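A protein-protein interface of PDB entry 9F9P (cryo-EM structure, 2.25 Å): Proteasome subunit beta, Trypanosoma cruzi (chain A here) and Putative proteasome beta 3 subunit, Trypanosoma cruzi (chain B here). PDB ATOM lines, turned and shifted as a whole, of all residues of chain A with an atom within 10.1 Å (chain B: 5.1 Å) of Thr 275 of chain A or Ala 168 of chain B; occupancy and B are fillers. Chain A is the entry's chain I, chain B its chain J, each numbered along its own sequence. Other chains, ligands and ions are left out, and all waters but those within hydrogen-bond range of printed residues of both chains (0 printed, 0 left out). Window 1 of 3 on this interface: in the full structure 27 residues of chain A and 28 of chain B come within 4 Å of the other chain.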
ATOM      1  N   PHE A 270      17.950  16.852 -23.106  1.00  0.00           N
ATOM      2  CA  PHE A 270      19.192  17.603 -22.988  1.00  0.00           C
ATOM      3  C   PHE A 270      19.645  17.547 -21.532  1.00  0.00           C
ATOM      4  O   PHE A 270      18.918  18.001 -20.647  1.00  0.00           O
ATOM      5  CB  PHE A 270      19.045  19.049 -23.491  1.00  0.00           C
ATOM      6  CG  PHE A 270      18.906  19.164 -24.990  1.00  0.00           C
ATOM      7  CD1 PHE A 270      19.892  18.661 -25.832  1.00  0.00           C
ATOM      8  CD2 PHE A 270      17.772  19.719 -25.566  1.00  0.00           C
ATOM      9  CE1 PHE A 270      19.754  18.713 -27.211  1.00  0.00           C
ATOM     10  CE2 PHE A 270      17.642  19.777 -26.945  1.00  0.00           C
ATOM     11  CZ  PHE A 270      18.631  19.277 -27.765  1.00  0.00           C
ATOM     12  N   PRO A 271      20.834  16.953 -21.250  1.00  0.00           N
ATOM     13  CA  PRO A 271      21.440  16.969 -19.911  1.00  0.00           C
ATOM     14  C   PRO A 271      21.598  18.374 -19.319  1.00  0.00           C
ATOM     15  O   PRO A 271      22.134  19.250 -19.992  1.00  0.00           O
ATOM     16  CB  PRO A 271      22.840  16.374 -20.148  1.00  0.00           C
ATOM     17  CG  PRO A 271      22.699  15.514 -21.387  1.00  0.00           C
ATOM     18  CD  PRO A 271      21.658  16.218 -22.229  1.00  0.00           C
ATOM     19  N   PRO A 272      21.140  18.665 -18.073  1.00  0.00           N
ATOM     20  CA  PRO A 272      21.305  20.003 -17.480  1.00  0.00           C
ATOM     21  C   PRO A 272      22.769  20.427 -17.315  1.00  0.00           C
ATOM     22  O   PRO A 272      23.557  19.707 -16.707  1.00  0.00           O
ATOM     23  CB  PRO A 272      20.584  19.913 -16.118  1.00  0.00           C
ATOM     24  CG  PRO A 272      19.663  18.708 -16.248  1.00  0.00           C
ATOM     25  CD  PRO A 272      20.375  17.760 -17.195  1.00  0.00           C
ATOM     26  N   GLY A 273      23.110  21.606 -17.871  1.00  0.00           N
ATOM     27  CA  GLY A 273      24.487  22.072 -18.028  1.00  0.00           C
ATOM     28  C   GLY A 273      24.965  22.090 -19.489  1.00  0.00           C
ATOM     29  O   GLY A 273      26.081  22.531 -19.764  1.00  0.00           O
ATOM     30  N   THR A 274      24.098  21.636 -20.419  1.00  0.00           N
ATOM     31  CA  THR A 274      24.379  21.504 -21.851  1.00  0.00           C
ATOM     32  C   THR A 274      24.717  22.846 -22.514  1.00  0.00           C
ATOM     33  O   THR A 274      25.599  22.910 -23.365  1.00  0.00           O
ATOM     34  CB  THR A 274      23.182  20.864 -22.578  1.00  0.00           C
ATOM     35  OG1 THR A 274      22.975  19.551 -22.056  1.00  0.00           O
ATOM     36  CG2 THR A 274      23.362  20.758 -24.077  1.00  0.00           C
ATOM     37  N   THR A 275      23.988  23.906 -22.142  1.00  0.00           N
ATOM     38  CA  THR A 275      24.111  25.214 -22.774  1.00  0.00           C
ATOM     39  C   THR A 275      25.191  26.048 -22.074  1.00  0.00           C
ATOM     40  O   THR A 275      25.195  26.148 -20.849  1.00  0.00           O
ATOM     41  CB  THR A 275      22.737  25.902 -22.799  1.00  0.00           C
ATOM     42  OG1 THR A 275      21.786  25.006 -23.390  1.00  0.00           O
ATOM     43  CG2 THR A 275      22.772  27.214 -23.552  1.00  0.00           C
ATOM     44  N   PRO A 276      26.153  26.664 -22.808  1.00  0.00           N
ATOM     45  CA  PRO A 276      27.115  27.599 -22.209  1.00  0.00           C
ATOM     46  C   PRO A 276      26.531  28.953 -21.810  1.00  0.00           C
ATOM     47  O   PRO A 276      25.892  29.622 -22.615  1.00  0.00           O
ATOM     48  CB  PRO A 276      28.182  27.815 -23.295  1.00  0.00           C
ATOM     49  CG  PRO A 276      27.956  26.669 -24.264  1.00  0.00           C
ATOM     50  CD  PRO A 276      26.459  26.420 -24.226  1.00  0.00           C
ATOM     51  N   VAL A 277      26.794  29.343 -20.557  1.00  0.00           N
ATOM     52  CA  VAL A 277      26.298  30.571 -19.956  1.00  0.00           C
ATOM     53  C   VAL A 277      27.506  31.435 -19.590  1.00  0.00           C
ATOM     54  O   VAL A 277      28.521  30.902 -19.143  1.00  0.00           O
ATOM     55  CB  VAL A 277      25.421  30.245 -18.727  1.00  0.00           C
ATOM     56  CG1 VAL A 277      25.113  31.479 -17.891  1.00  0.00           C
ATOM     57  CG2 VAL A 277      24.131  29.524 -19.109  1.00  0.00           C
ATOM     58  N   LEU A 278      27.388  32.762 -19.779  1.00  0.00           N
ATOM     59  CA  LEU A 278      28.456  33.702 -19.453  1.00  0.00           C
ATOM     60  C   LEU A 278      28.218  34.375 -18.098  1.00  0.00           C
ATOM     61  O   LEU A 278      29.185  34.685 -17.407  1.00  0.00           O
ATOM     62  CB  LEU A 278      28.577  34.765 -20.556  1.00  0.00           C
ATOM     63  CG  LEU A 278      28.974  34.276 -21.955  1.00  0.00           C
ATOM     64  CD1 LEU A 278      28.745  35.366 -23.010  1.00  0.00           C
ATOM     65  CD2 LEU A 278      30.424  33.786 -21.981  1.00  0.00           C
ATOM     66  N   ARG A 279      26.948  34.640 -17.735  1.00  0.00           N
ATOM     67  CA  ARG A 279      26.617  35.433 -16.553  1.00  0.00           C
ATOM     68  C   ARG A 279      25.218  35.091 -16.044  1.00  0.00           C
ATOM     69  O   ARG A 279      24.390  34.551 -16.777  1.00  0.00           O
ATOM     70  CB  ARG A 279      26.626  36.943 -16.822  1.00  0.00           C
ATOM     71  CG  ARG A 279      27.967  37.549 -17.199  1.00  0.00           C
ATOM     72  CD  ARG A 279      28.008  39.019 -16.811  1.00  0.00           C
ATOM     73  NE  ARG A 279      28.565  39.852 -17.869  1.00  0.00           N
ATOM     74  CZ  ARG A 279      27.944  40.894 -18.420  1.00  0.00           C
ATOM     75  NH1 ARG A 279      26.789  41.319 -17.935  1.00  0.00           N
ATOM     76  NH2 ARG A 279      28.490  41.523 -19.449  1.00  0.00           N
ATOM     77  N   GLU A 280      24.970  35.468 -14.782  1.00  0.00           N
ATOM     78  CA  GLU A 280      23.762  35.094 -14.061  1.00  0.00           C
ATOM     79  C   GLU A 280      23.467  36.130 -12.971  1.00  0.00           C
ATOM     80  O   GLU A 280      24.375  36.568 -12.262  1.00  0.00           O
ATOM     81  CB  GLU A 280      23.917  33.673 -13.508  1.00  0.00           C
ATOM     82  CG  GLU A 280      22.704  33.162 -12.741  1.00  0.00           C
ATOM     83  CD  GLU A 280      22.637  31.650 -12.575  1.00  0.00           C
ATOM     84  OE1 GLU A 280      22.366  30.961 -13.580  1.00  0.00           O
ATOM     85  OE2 GLU A 280      22.876  31.157 -11.443  1.00  0.00           O
ATOM     86  N   VAL B  23      12.821  34.202 -23.637  1.00  0.00           N
ATOM     87  CA  VAL B  23      14.159  34.368 -24.204  1.00  0.00           C
ATOM     88  C   VAL B  23      14.111  35.344 -25.376  1.00  0.00           C
ATOM     89  O   VAL B  23      13.179  35.289 -26.166  1.00  0.00           O
ATOM     90  CB  VAL B  23      14.735  33.038 -24.732  1.00  0.00           C
ATOM     91  CG1 VAL B  23      16.205  33.132 -25.080  1.00  0.00           C
ATOM     92  CG2 VAL B  23      14.649  31.915 -23.745  1.00  0.00           C
ATOM     93  N   PHE B 164      14.826  25.527 -19.110  1.00  0.00           N
ATOM     94  CA  PHE B 164      15.804  26.480 -19.593  1.00  0.00           C
ATOM     95  C   PHE B 164      16.635  25.915 -20.755  1.00  0.00           C
ATOM     96  O   PHE B 164      16.778  26.604 -21.772  1.00  0.00           O
ATOM     97  CB  PHE B 164      16.704  26.942 -18.455  1.00  0.00           C
ATOM     98  CG  PHE B 164      17.876  27.747 -18.942  1.00  0.00           C
ATOM     99  CD1 PHE B 164      17.695  29.032 -19.412  1.00  0.00           C
ATOM    100  CD2 PHE B 164      19.144  27.193 -19.004  1.00  0.00           C
ATOM    101  CE1 PHE B 164      18.772  29.764 -19.909  1.00  0.00           C
ATOM    102  CE2 PHE B 164      20.215  27.932 -19.489  1.00  0.00           C
ATOM    103  CZ  PHE B 164      20.028  29.218 -19.953  1.00  0.00           C
ATOM    104  N   GLU B 165      17.154  24.680 -20.615  1.00  0.00           N
ATOM    105  CA  GLU B 165      17.959  24.041 -21.655  1.00  0.00           C
ATOM    106  C   GLU B 165      17.250  23.934 -22.995  1.00  0.00           C
ATOM    107  O   GLU B 165      17.835  24.159 -24.045  1.00  0.00           O
ATOM    108  CB  GLU B 165      18.333  22.607 -21.301  1.00  0.00           C
ATOM    109  CG  GLU B 165      19.259  22.534 -20.103  1.00  0.00           C
ATOM    110  CD  GLU B 165      20.442  23.497 -20.164  1.00  0.00           C
ATOM    111  OE1 GLU B 165      20.851  24.029 -19.095  1.00  0.00           O
ATOM    112  OE2 GLU B 165      20.962  23.723 -21.281  1.00  0.00           O
ATOM    113  N   VAL B 166      15.985  23.572 -22.954  1.00  0.00           N
ATOM    114  CA  VAL B 166      15.211  23.397 -24.161  1.00  0.00           C
ATOM    115  C   VAL B 166      15.000  24.755 -24.841  1.00  0.00           C
ATOM    116  O   VAL B 166      15.018  24.832 -26.067  1.00  0.00           O
ATOM    117  CB  VAL B 166      13.886  22.726 -23.775  1.00  0.00           C
ATOM    118  CG1 VAL B 166      12.750  22.988 -24.762  1.00  0.00           C
ATOM    119  CG2 VAL B 166      14.082  21.250 -23.556  1.00  0.00           C
ATOM    120  N   ALA B 167      14.738  25.822 -24.069  1.00  0.00           N
ATOM    121  CA  ALA B 167      14.462  27.111 -24.684  1.00  0.00           C
ATOM    122  C   ALA B 167      15.735  27.724 -25.280  1.00  0.00           C
ATOM    123  O   ALA B 167      15.704  28.372 -26.311  1.00  0.00           O
ATOM    124  CB  ALA B 167      13.838  28.058 -23.687  1.00  0.00           C
ATOM    125  N   ALA B 168      16.863  27.551 -24.608  1.00  0.00           N
ATOM    126  CA  ALA B 168      18.106  28.055 -25.148  1.00  0.00           C
ATOM    127  C   ALA B 168      18.453  27.347 -26.459  1.00  0.00           C
ATOM    128  O   ALA B 168      18.792  27.997 -27.423  1.00  0.00           O
ATOM    129  CB  ALA B 168      19.190  27.905 -24.112  1.00  0.00           C
ATOM    130  N   GLN B 169      18.375  26.018 -26.521  1.00  0.00           N
ATOM    131  CA  GLN B 169      18.700  25.311 -27.750  1.00  0.00           C
ATOM    132  C   GLN B 169      17.758  25.700 -28.893  1.00  0.00           C
ATOM    133  O   GLN B 169      18.169  25.705 -30.052  1.00  0.00           O
ATOM    134  CB  GLN B 169      18.645  23.790 -27.562  1.00  0.00           C
ATOM    135  CG  GLN B 169      19.797  23.248 -26.732  1.00  0.00           C
ATOM    136  CD  GLN B 169      21.177  23.584 -27.279  1.00  0.00           C
ATOM    137  OE1 GLN B 169      21.516  23.313 -28.436  1.00  0.00           O
ATOM    138  NE2 GLN B 169      22.001  24.202 -26.447  1.00  0.00           N
ATOM    139  N   ALA B 170      16.488  25.937 -28.596  1.00  0.00           N
ATOM    140  CA  ALA B 170      15.580  26.315 -29.653  1.00  0.00           C
ATOM    141  C   ALA B 170      15.969  27.692 -30.198  1.00  0.00           C
ATOM    142  O   ALA B 170      15.934  27.912 -31.410  1.00  0.00           O
ATOM    143  CB  ALA B 170      14.144  26.337 -29.162  1.00  0.00           C
ATOM    144  N   MET B 171      16.336  28.622 -29.308  1.00  0.00           N
ATOM    145  CA  MET B 171      16.619  29.972 -29.747  1.00  0.00           C
ATOM    146  C   MET B 171      17.919  29.974 -30.549  1.00  0.00           C
ATOM    147  O   MET B 171      17.948  30.603 -31.602  1.00  0.00           O
ATOM    148  CB  MET B 171      16.658  30.947 -28.564  1.00  0.00           C
ATOM    149  CG  MET B 171      17.013  32.423 -28.908  1.00  0.00           C
ATOM    150  SD  MET B 171      15.923  33.325 -30.077  1.00  0.00           S
ATOM    151  CE  MET B 171      14.475  33.704 -29.101  1.00  0.00           C
ATOM    152  N   LEU B 172      18.964  29.251 -30.111  1.00  0.00           N
ATOM    153  CA  LEU B 172      20.243  29.253 -30.826  1.00  0.00           C
ATOM    154  C   LEU B 172      20.196  28.525 -32.172  1.00  0.00           C
ATOM    155  O   LEU B 172      20.851  28.952 -33.114  1.00  0.00           O
ATOM    156  CB  LEU B 172      21.322  28.602 -29.964  1.00  0.00           C
ATOM    157  CG  LEU B 172      21.630  29.383 -28.691  1.00  0.00           C
ATOM    158  CD1 LEU B 172      22.640  28.666 -27.820  1.00  0.00           C
ATOM    159  CD2 LEU B 172      22.102  30.802 -29.010  1.00  0.00           C
ATOM    160  N   SER B 173      19.462  27.427 -32.284  1.00  0.00           N
ATOM    161  CA  SER B 173      19.359  26.769 -33.569  1.00  0.00           C
ATOM    162  C   SER B 173      18.613  27.626 -34.584  1.00  0.00           C
ATOM    163  O   SER B 173      18.973  27.661 -35.750  1.00  0.00           O
ATOM    164  CB  SER B 173      18.692  25.438 -33.435  1.00  0.00           C
ATOM    165  OG  SER B 173      19.332  24.724 -32.401  1.00  0.00           O
ATOM    166  N   ILE B 200      23.265  33.941 -22.427  1.00  0.00           N
ATOM    167  CA  ILE B 200      23.625  32.751 -23.179  1.00  0.00           C
ATOM    168  C   ILE B 200      24.604  33.152 -24.277  1.00  0.00           C
ATOM    169  O   ILE B 200      24.321  34.073 -25.039  1.00  0.00           O
ATOM    170  CB  ILE B 200      22.357  32.165 -23.830  1.00  0.00           C
ATOM    171  CG1 ILE B 200      21.207  32.062 -22.839  1.00  0.00           C
ATOM    172  CG2 ILE B 200      22.641  30.841 -24.497  1.00  0.00           C
ATOM    173  CD1 ILE B 200      19.875  31.759 -23.469  1.00  0.00           C
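The side-chain carboxylate (OE2) of Glu 165 of chain B sits at hydrogen-bond distance from the side-chain hydroxyl (OG1) of Thr 275 of chain A (2.6 Å). OG1 of Thr 275 of chain A sits at hydrogen-bond distance from NE2 of Gln 169 of chain B (3.2 Å).
Among the printed residues, merely in contact across the chains: Gly 273 of chain A with Glu 165 of chain B (3.5 Å), Thr 274 of chain A with Glu 165 of chain B (3.8 Å), Thr 275 of chain A with Ala 168 of chain B (3.7 Å), Thr 275 of chain A with Ile 200 of chain B (3.8 Å) and Pro 276 of chain A with Ile 200 of chain B (3.9 Å).
Of chain A, only Thr 275 (3.7 Å) comes within 4 Å of Ala 168 of chain B. Of chain A, only Gly 273, Thr 274 and Thr 275 come within 4 Å of Glu 165 of chain B. No residue of chain A comes within 4 Å of Ala 170 of chain B. Of the printed residues of chain B, Thr 274 of chain A touches Glu 165 (3.8 Å). Printed residues of chain B within 4 Å of Pro 276 of chain A: Ile 200 (3.9 Å). Printed residues of chain B within 4 Å of Gly 273 of chain A: Glu 165 (3.5 Å). Met 171 of chain B touches none of the printed residues of chain A. The nearest residue of chain A that does not touch Ala 168 of chain B is Pro 276 of chain A (7.1 Å). The nearest printed residue of chain B that does not touch Gly 273 of chain A is Phe 164 of chain B (6.9 Å).
The backbone carbonyl oxygen (O) of Gln 169 of chain B lies within hydrogen-bond range of the side-chain hydroxyl (OG) of Ser 173 of chain B (2.8 Å).
Of the 12 printed residues of chain B, 4 touch a printed residue of chain A. Among the printed residues, no Asp or Glu carboxylate lies within 4 Å of a Lys or Arg side-chain nitrogen of the other chain.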
